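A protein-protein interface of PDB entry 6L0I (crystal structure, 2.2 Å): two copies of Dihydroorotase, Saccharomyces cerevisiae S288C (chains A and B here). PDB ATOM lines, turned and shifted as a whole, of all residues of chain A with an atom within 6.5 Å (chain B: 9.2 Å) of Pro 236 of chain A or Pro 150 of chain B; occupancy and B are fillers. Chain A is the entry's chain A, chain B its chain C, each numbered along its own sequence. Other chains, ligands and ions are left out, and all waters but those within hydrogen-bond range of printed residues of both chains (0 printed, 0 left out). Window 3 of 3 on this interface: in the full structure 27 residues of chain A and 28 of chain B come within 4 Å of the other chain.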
ATOM      1  N   THR A 217      27.698   5.230   1.806  1.00  0.00           N
ATOM      2  CA  THR A 217      28.659   5.688   0.804  1.00  0.00           C
ATOM      3  C   THR A 217      29.918   6.127   1.532  1.00  0.00           C
ATOM      4  O   THR A 217      29.974   6.133   2.763  1.00  0.00           O
ATOM      5  CB  THR A 217      28.146   6.863  -0.035  1.00  0.00           C
ATOM      6  OG1 THR A 217      27.968   7.981   0.825  1.00  0.00           O
ATOM      7  CG2 THR A 217      26.815   6.543  -0.758  1.00  0.00           C
ATOM      8  N   ILE A 218      30.938   6.518   0.763  1.00  0.00           N
ATOM      9  CA  ILE A 218      32.179   7.028   1.359  1.00  0.00           C
ATOM     10  C   ILE A 218      31.917   8.201   2.309  1.00  0.00           C
ATOM     11  O   ILE A 218      32.615   8.367   3.321  1.00  0.00           O
ATOM     12  CB  ILE A 218      33.178   7.414   0.251  1.00  0.00           C
ATOM     13  CG1 ILE A 218      34.516   7.836   0.860  1.00  0.00           C
ATOM     14  CG2 ILE A 218      32.604   8.516  -0.650  1.00  0.00           C
ATOM     15  CD1 ILE A 218      35.621   7.956  -0.143  1.00  0.00           C
ATOM     16  N   LYS A 234      31.593   2.858  -1.313  1.00  0.00           N
ATOM     17  CA  LYS A 234      32.153   3.642  -2.415  1.00  0.00           C
ATOM     18  C   LYS A 234      31.190   4.764  -2.779  1.00  0.00           C
ATOM     19  O   LYS A 234      30.686   5.431  -1.872  1.00  0.00           O
ATOM     20  CB  LYS A 234      32.527   2.685  -3.539  1.00  0.00           C
ATOM     21  CG  LYS A 234      33.744   1.799  -3.160  1.00  0.00           C
ATOM     22  CD  LYS A 234      33.934   0.612  -4.079  1.00  0.00           C
ATOM     23  CE  LYS A 234      35.218  -0.183  -3.706  1.00  0.00           C
ATOM     24  NZ  LYS A 234      35.097  -0.896  -2.370  1.00  0.00           N
ATOM     25  N   LEU A 235      30.917   5.008  -4.017  1.00  0.00           N
ATOM     26  CA  LEU A 235      30.265   6.220  -4.452  1.00  0.00           C
ATOM     27  C   LEU A 235      28.756   6.022  -4.555  1.00  0.00           C
ATOM     28  O   LEU A 235      28.265   4.888  -4.537  1.00  0.00           O
ATOM     29  CB  LEU A 235      30.855   6.644  -5.802  1.00  0.00           C
ATOM     30  CG  LEU A 235      32.378   6.767  -5.698  1.00  0.00           C
ATOM     31  CD1 LEU A 235      33.010   7.108  -7.037  1.00  0.00           C
ATOM     32  CD2 LEU A 235      32.712   7.835  -4.670  1.00  0.00           C
ATOM     33  N   PRO A 236      27.980   7.117  -4.631  1.00  0.00           N
ATOM     34  CA  PRO A 236      26.528   6.969  -4.857  1.00  0.00           C
ATOM     35  C   PRO A 236      26.192   6.107  -6.063  1.00  0.00           C
ATOM     36  O   PRO A 236      25.254   5.313  -5.997  1.00  0.00           O
ATOM     37  CB  PRO A 236      26.064   8.420  -5.038  1.00  0.00           C
ATOM     38  CG  PRO A 236      27.063   9.226  -4.253  1.00  0.00           C
ATOM     39  CD  PRO A 236      28.370   8.533  -4.470  1.00  0.00           C
ATOM     40  N   ASN A 237      26.965   6.216  -7.150  1.00  0.00           N
ATOM     41  CA  ASN A 237      26.779   5.355  -8.324  1.00  0.00           C
ATOM     42  C   ASN A 237      26.976   3.873  -7.998  1.00  0.00           C
ATOM     43  O   ASN A 237      26.345   3.009  -8.627  1.00  0.00           O
ATOM     44  CB  ASN A 237      27.741   5.781  -9.432  1.00  0.00           C
ATOM     45  CG  ASN A 237      27.633   4.907 -10.685  1.00  0.00           C
ATOM     46  OD1 ASN A 237      26.595   4.874 -11.358  1.00  0.00           O
ATOM     47  ND2 ASN A 237      28.708   4.193 -11.000  1.00  0.00           N
ATOM     48  N   ASP A 238      27.850   3.554  -7.038  1.00  0.00           N
ATOM     49  CA  ASP A 238      28.040   2.160  -6.660  1.00  0.00           C
ATOM     50  C   ASP A 238      26.891   1.661  -5.800  1.00  0.00           C
ATOM     51  O   ASP A 238      26.356   0.574  -6.041  1.00  0.00           O
ATOM     52  CB  ASP A 238      29.359   1.996  -5.920  1.00  0.00           C
ATOM     53  CG  ASP A 238      30.532   2.399  -6.757  1.00  0.00           C
ATOM     54  OD1 ASP A 238      30.745   1.772  -7.812  1.00  0.00           O
ATOM     55  OD2 ASP A 238      31.232   3.361  -6.379  1.00  0.00           O
ATOM     56  N   LYS A 239      26.504   2.441  -4.789  1.00  0.00           N
ATOM     57  CA  LYS A 239      25.384   2.050  -3.947  1.00  0.00           C
ATOM     58  C   LYS A 239      24.096   1.891  -4.748  1.00  0.00           C
ATOM     59  O   LYS A 239      23.217   1.109  -4.359  1.00  0.00           O
ATOM     60  CB  LYS A 239      25.175   3.080  -2.846  1.00  0.00           C
ATOM     61  CG  LYS A 239      24.050   2.725  -1.899  1.00  0.00           C
ATOM     62  CD  LYS A 239      23.969   3.713  -0.761  1.00  0.00           C
ATOM     63  CE  LYS A 239      23.085   4.869  -1.103  1.00  0.00           C
ATOM     64  NZ  LYS A 239      22.225   5.152   0.080  1.00  0.00           N
ATOM     65  N   LYS A 240      23.950   2.649  -5.843  1.00  0.00           N
ATOM     66  CA  LYS A 240      22.767   2.517  -6.689  1.00  0.00           C
ATOM     67  C   LYS A 240      22.767   1.173  -7.399  1.00  0.00           C
ATOM     68  O   LYS A 240      21.734   0.501  -7.449  1.00  0.00           O
ATOM     69  CB  LYS A 240      22.696   3.671  -7.701  1.00  0.00           C
ATOM     70  CG  LYS A 240      21.907   3.363  -8.995  1.00  0.00           C
ATOM     71  CD  LYS A 240      22.348   4.259 -10.161  1.00  0.00           C
ATOM     72  CE  LYS A 240      21.306   4.342 -11.295  1.00  0.00           C
ATOM     73  NZ  LYS A 240      21.439   3.303 -12.394  1.00  0.00           N
ATOM     74  N   ALA A 241      23.925   0.747  -7.920  1.00  0.00           N
ATOM     75  CA  ALA A 241      24.023  -0.584  -8.515  1.00  0.00           C
ATOM     76  C   ALA A 241      23.805  -1.681  -7.479  1.00  0.00           C
ATOM     77  O   ALA A 241      23.143  -2.685  -7.760  1.00  0.00           O
ATOM     78  CB  ALA A 241      25.375  -0.769  -9.195  1.00  0.00           C
ATOM     79  N   LYS B 140      31.751  21.886  -2.775  1.00  0.00           N
ATOM     80  CA  LYS B 140      30.302  21.958  -2.734  1.00  0.00           C
ATOM     81  C   LYS B 140      29.783  21.031  -1.638  1.00  0.00           C
ATOM     82  O   LYS B 140      30.326  19.942  -1.440  1.00  0.00           O
ATOM     83  CB  LYS B 140      29.704  21.563  -4.087  1.00  0.00           C
ATOM     84  CG  LYS B 140      29.649  22.685  -5.106  1.00  0.00           C
ATOM     85  CD  LYS B 140      28.197  23.138  -5.363  1.00  0.00           C
ATOM     86  CE  LYS B 140      28.085  24.125  -6.550  1.00  0.00           C
ATOM     87  NZ  LYS B 140      28.949  25.343  -6.397  1.00  0.00           N
ATOM     88  N   PRO B 141      28.760  21.444  -0.894  1.00  0.00           N
ATOM     89  CA  PRO B 141      28.136  20.532   0.075  1.00  0.00           C
ATOM     90  C   PRO B 141      27.621  19.264  -0.594  1.00  0.00           C
ATOM     91  O   PRO B 141      27.202  19.274  -1.750  1.00  0.00           O
ATOM     92  CB  PRO B 141      26.989  21.367   0.648  1.00  0.00           C
ATOM     93  CG  PRO B 141      27.495  22.770   0.555  1.00  0.00           C
ATOM     94  CD  PRO B 141      28.311  22.829  -0.717  1.00  0.00           C
ATOM     95  N   SER B 142      27.663  18.159   0.152  1.00  0.00           N
ATOM     96  CA  SER B 142      27.321  16.851  -0.399  1.00  0.00           C
ATOM     97  C   SER B 142      25.819  16.738  -0.633  1.00  0.00           C
ATOM     98  O   SER B 142      25.013  17.102   0.231  1.00  0.00           O
ATOM     99  CB  SER B 142      27.788  15.732   0.541  1.00  0.00           C
ATOM    100  OG  SER B 142      29.186  15.456   0.423  1.00  0.00           O
ATOM    101  N   VAL B 143      25.443  16.233  -1.810  1.00  0.00           N
ATOM    102  CA  VAL B 143      24.050  15.953  -2.151  1.00  0.00           C
ATOM    103  C   VAL B 143      24.005  14.587  -2.820  1.00  0.00           C
ATOM    104  O   VAL B 143      24.805  14.309  -3.721  1.00  0.00           O
ATOM    105  CB  VAL B 143      23.436  17.032  -3.072  1.00  0.00           C
ATOM    106  CG1 VAL B 143      23.250  18.345  -2.329  1.00  0.00           C
ATOM    107  CG2 VAL B 143      24.298  17.251  -4.288  1.00  0.00           C
ATOM    108  N   HIS B 144      23.084  13.726  -2.381  1.00  0.00           N
ATOM    109  CA  HIS B 144      23.028  12.366  -2.906  1.00  0.00           C
ATOM    110  C   HIS B 144      21.755  12.040  -3.677  1.00  0.00           C
ATOM    111  O   HIS B 144      21.798  11.192  -4.575  1.00  0.00           O
ATOM    112  CB  HIS B 144      23.210  11.347  -1.768  1.00  0.00           C
ATOM    113  CG  HIS B 144      24.621  11.247  -1.272  1.00  0.00           C
ATOM    114  ND1 HIS B 144      24.978  10.488  -0.178  1.00  0.00           N
ATOM    115  CD2 HIS B 144      25.763  11.824  -1.718  1.00  0.00           C
ATOM    116  CE1 HIS B 144      26.280  10.599   0.026  1.00  0.00           C
ATOM    117  NE2 HIS B 144      26.779  11.407  -0.892  1.00  0.00           N
ATOM    118  N   ASP B 145      20.635  12.696  -3.369  1.00  0.00           N
ATOM    119  CA  ASP B 145      19.386  12.460  -4.085  1.00  0.00           C
ATOM    120  C   ASP B 145      19.440  13.099  -5.478  1.00  0.00           C
ATOM    121  O   ASP B 145      20.445  13.695  -5.887  1.00  0.00           O
ATOM    122  CB  ASP B 145      18.203  12.996  -3.276  1.00  0.00           C
ATOM    123  CG  ASP B 145      18.488  14.356  -2.638  1.00  0.00           C
ATOM    124  OD1 ASP B 145      19.617  14.562  -2.148  1.00  0.00           O
ATOM    125  OD2 ASP B 145      17.582  15.219  -2.624  1.00  0.00           O
ATOM    126  N   GLY B 146      18.345  12.960  -6.224  1.00  0.00           N
ATOM    127  CA  GLY B 146      18.184  13.705  -7.460  1.00  0.00           C
ATOM    128  C   GLY B 146      18.217  15.200  -7.194  1.00  0.00           C
ATOM    129  O   GLY B 146      18.182  15.661  -6.054  1.00  0.00           O
ATOM    130  N   ASP B 147      18.292  15.987  -8.262  1.00  0.00           N
ATOM    131  CA  ASP B 147      18.180  15.575  -9.655  1.00  0.00           C
ATOM    132  C   ASP B 147      19.558  15.374 -10.285  1.00  0.00           C
ATOM    133  O   ASP B 147      19.746  14.473 -11.114  1.00  0.00           O
ATOM    134  CB  ASP B 147      17.396  16.668 -10.400  1.00  0.00           C
ATOM    135  CG  ASP B 147      17.153  16.344 -11.857  1.00  0.00           C
ATOM    136  OD1 ASP B 147      16.012  15.961 -12.190  1.00  0.00           O
ATOM    137  OD2 ASP B 147      18.087  16.502 -12.669  1.00  0.00           O
ATOM    138  N   LYS B 148      20.510  16.195  -9.849  1.00  0.00           N
ATOM    139  CA  LYS B 148      21.808  16.405 -10.480  1.00  0.00           C
ATOM    140  C   LYS B 148      22.699  15.169 -10.329  1.00  0.00           C
ATOM    141  O   LYS B 148      22.266  14.092  -9.907  1.00  0.00           O
ATOM    142  CB  LYS B 148      22.473  17.642  -9.903  1.00  0.00           C
ATOM    143  CG  LYS B 148      21.821  18.953 -10.310  1.00  0.00           C
ATOM    144  CD  LYS B 148      21.430  19.802  -9.104  1.00  0.00           C
ATOM    145  CE  LYS B 148      20.752  21.090  -9.554  1.00  0.00           C
ATOM    146  NZ  LYS B 148      21.634  21.864 -10.477  1.00  0.00           N
ATOM    147  N   GLU B 149      23.977  15.323 -10.664  1.00  0.00           N
ATOM    148  CA  GLU B 149      24.971  14.297 -10.375  1.00  0.00           C
ATOM    149  C   GLU B 149      25.398  14.407  -8.913  1.00  0.00           C
ATOM    150  O   GLU B 149      25.659  15.514  -8.435  1.00  0.00           O
ATOM    151  CB  GLU B 149      26.178  14.438 -11.302  1.00  0.00           C
ATOM    152  CG  GLU B 149      26.036  13.692 -12.639  1.00  0.00           C
ATOM    153  CD  GLU B 149      27.277  12.890 -13.010  1.00  0.00           C
ATOM    154  OE1 GLU B 149      27.443  11.780 -12.462  1.00  0.00           O
ATOM    155  OE2 GLU B 149      28.081  13.365 -13.846  1.00  0.00           O
ATOM    156  N   PRO B 150      25.467  13.294  -8.180  1.00  0.00           N
ATOM    157  CA  PRO B 150      25.640  13.369  -6.720  1.00  0.00           C
ATOM    158  C   PRO B 150      26.989  13.958  -6.320  1.00  0.00           C
ATOM    159  O   PRO B 150      27.996  13.801  -7.019  1.00  0.00           O
ATOM    160  CB  PRO B 150      25.517  11.906  -6.270  1.00  0.00           C
ATOM    161  CG  PRO B 150      24.866  11.189  -7.407  1.00  0.00           C
ATOM    162  CD  PRO B 150      25.305  11.907  -8.649  1.00  0.00           C
ATOM    163  N   ILE B 151      26.989  14.668  -5.185  1.00  0.00           N
ATOM    164  CA  ILE B 151      28.185  15.302  -4.632  1.00  0.00           C
ATOM    165  C   ILE B 151      28.626  14.512  -3.411  1.00  0.00           C
ATOM    166  O   ILE B 151      27.834  14.299  -2.486  1.00  0.00           O
ATOM    167  CB  ILE B 151      27.948  16.775  -4.245  1.00  0.00           C
ATOM    168  CG1 ILE B 151      27.616  17.639  -5.460  1.00  0.00           C
ATOM    169  CG2 ILE B 151      29.178  17.330  -3.527  1.00  0.00           C
ATOM    170  CD1 ILE B 151      28.420  17.299  -6.659  1.00  0.00           C
ATOM    171  N   HIS B 152      29.898  14.110  -3.390  1.00  0.00           N
ATOM    172  CA  HIS B 152      30.465  13.365  -2.275  1.00  0.00           C
ATOM    173  C   HIS B 152      31.872  13.906  -1.985  1.00  0.00           C
ATOM    174  O   HIS B 152      32.377  14.781  -2.693  1.00  0.00           O
ATOM    175  CB  HIS B 152      30.463  11.875  -2.602  1.00  0.00           C
ATOM    176  CG  HIS B 152      31.072  11.574  -3.931  1.00  0.00           C
ATOM    177  ND1 HIS B 152      32.434  11.538  -4.130  1.00  0.00           N
ATOM    178  CD2 HIS B 152      30.510  11.340  -5.142  1.00  0.00           C
ATOM    179  CE1 HIS B 152      32.687  11.288  -5.403  1.00  0.00           C
ATOM    180  NE2 HIS B 152      31.537  11.157  -6.038  1.00  0.00           N
ATOM    181  N   VAL B 153      32.524  13.385  -0.933  1.00  0.00           N
ATOM    182  CA  VAL B 153      33.801  13.953  -0.493  1.00  0.00           C
ATOM    183  C   VAL B 153      34.888  13.817  -1.554  1.00  0.00           C
ATOM    184  O   VAL B 153      35.880  14.556  -1.505  1.00  0.00           O
ATOM    185  CB  VAL B 153      34.285  13.337   0.850  1.00  0.00           C
ATOM    186  CG1 VAL B 153      33.261  13.545   1.953  1.00  0.00           C
ATOM    187  CG2 VAL B 153      34.600  11.864   0.691  1.00  0.00           C
ATOM    188  N   LEU B 154      34.723  12.926  -2.539  1.00  0.00           N
ATOM    189  CA  LEU B 154      35.746  12.794  -3.581  1.00  0.00           C
ATOM    190  C   LEU B 154      35.588  13.754  -4.759  1.00  0.00           C
ATOM    191  O   LEU B 154      36.602  14.165  -5.331  1.00  0.00           O
ATOM    192  CB  LEU B 154      35.779  11.369  -4.130  1.00  0.00           C
ATOM    193  CG  LEU B 154      36.307  10.393  -3.109  1.00  0.00           C
ATOM    194  CD1 LEU B 154      36.353   9.073  -3.757  1.00  0.00           C
ATOM    195  CD2 LEU B 154      37.680  10.805  -2.591  1.00  0.00           C
ATOM    196  N   ASN B 155      34.365  14.124  -5.150  1.00  0.00           N
ATOM    197  CA  ASN B 155      34.170  15.042  -6.274  1.00  0.00           C
ATOM    198  C   ASN B 155      33.703  16.429  -5.850  1.00  0.00           C
ATOM    199  O   ASN B 155      33.450  17.273  -6.721  1.00  0.00           O
ATOM    200  CB  ASN B 155      33.178  14.456  -7.284  1.00  0.00           C
ATOM    201  CG  ASN B 155      31.758  14.392  -6.748  1.00  0.00           C
ATOM    202  OD1 ASN B 155      31.476  14.758  -5.603  1.00  0.00           O
ATOM    203  ND2 ASN B 155      30.845  13.933  -7.588  1.00  0.00           N
ATOM    204  N   ALA B 156      33.608  16.691  -4.542  1.00  0.00           N
ATOM    205  CA  ALA B 156      33.083  17.966  -4.055  1.00  0.00           C
ATOM    206  C   ALA B 156      33.972  19.136  -4.451  1.00  0.00           C
ATOM    207  O   ALA B 156      33.472  20.244  -4.692  1.00  0.00           O
ATOM    208  CB  ALA B 156      32.917  17.926  -2.533  1.00  0.00           C
ATOM    209  N   GLU B 158      35.937  19.243  -7.306  1.00  0.00           N
ATOM    210  CA  GLU B 158      35.691  19.417  -8.731  1.00  0.00           C
ATOM    211  C   GLU B 158      34.356  20.110  -8.963  1.00  0.00           C
ATOM    212  O   GLU B 158      34.268  21.064  -9.739  1.00  0.00           O
ATOM    213  CB  GLU B 158      35.737  18.049  -9.405  1.00  0.00           C
ATOM    214  CG  GLU B 158      35.646  18.009 -10.907  1.00  0.00           C
ATOM    215  CD  GLU B 158      35.828  16.579 -11.424  1.00  0.00           C
ATOM    216  OE1 GLU B 158      36.976  16.186 -11.709  1.00  0.00           O
ATOM    217  OE2 GLU B 158      34.825  15.830 -11.510  1.00  0.00           O
ATOM    218  N   ALA B 159      33.315  19.675  -8.253  1.00  0.00           N
ATOM    219  CA  ALA B 159      31.999  20.276  -8.393  1.00  0.00           C
ATOM    220  C   ALA B 159      31.974  21.747  -7.996  1.00  0.00           C
ATOM    221  O   ALA B 159      31.051  22.468  -8.411  1.00  0.00           O
ATOM    222  CB  ALA B 159      30.992  19.506  -7.547  1.00  0.00           C
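Hydrophobic or aromatic side chains of chain A that line the printed part of chain B: Ile 218, Leu 235 and Pro 236. Among the printed residues, no Asp or Glu carboxylate lies within 4 Å of a Lys or Arg side-chain nitrogen of the other chain.
No position is printed for both chains. Of the 7 pairs that touch across the chains among the printed residues, none has its exchanged pair printed and touching as well.
The side-chain carboxylate (OD2) of Asp 238 of chain A lies within hydrogen-bond range of the backbone NH (N) of Leu 235 of chain A, at 2.9 Å. A ring nitrogen (NE2) of His 144 of chain B lies close to the backbone carbonyl oxygen (O) of Ile 151 of chain B (3.5 Å). N of Leu 154 of chain B sits close to ND1 of His 152 of chain B, at 3.1 Å. The backbone carbonyl oxygen (O) of Pro 150 of chain B is in hydrogen-bond range of the side-chain amide nitrogen (ND2) of Asn 155 of chain B (2.9 Å). The backbone carbonyl oxygen (O) of Lys 234 of chain A lies within hydrogen-bond range of the backbone NH (N) of Ile 218 of chain A. The backbone NH (N) of His 152 of chain B lies within hydrogen-bond range of the side-chain amide oxygen (OD1) of Asn 155 of chain B (2.8 Å).
Pro 150 of chain B touches just one residue of chain A: Pro 236 (3.7 Å). Of the printed residues of chain B, Thr 217 of chain A touches His 144 (3.2 Å). Printed residues of chain A within 4 Å of His 144 of chain B: Thr 217 and Pro 236. Of the printed residues of chain B, Leu 235 of chain A touches His 152 (3.5 Å) and Leu 154 (3.95 Å). The nearest residue of chain B that does not touch Pro 236 of chain A is Ile 151 of chain B (5.4 Å). The nearest residue of chain A that does not touch Pro 150 of chain B is Asn 237 of chain A (5.4 Å).
Among the printed residues, pairs that only touch across the chains: Thr 217 of chain A with His 144 of chain B (3.2 Å), Leu 235 of chain A with His 152 of chain B (3.5 Å), Pro 236 of chain A with His 152 of chain B (3.6 Å), Pro 236 of chain A with Pro 150 of chain B (3.7 Å), Ile 218 of chain A with Leu 154 of chain B (3.9 Å), Pro 236 of chain A with His 144 of chain B (3.9 Å) and Leu 235 of chain A with Leu 154 of chain B (3.95 Å).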
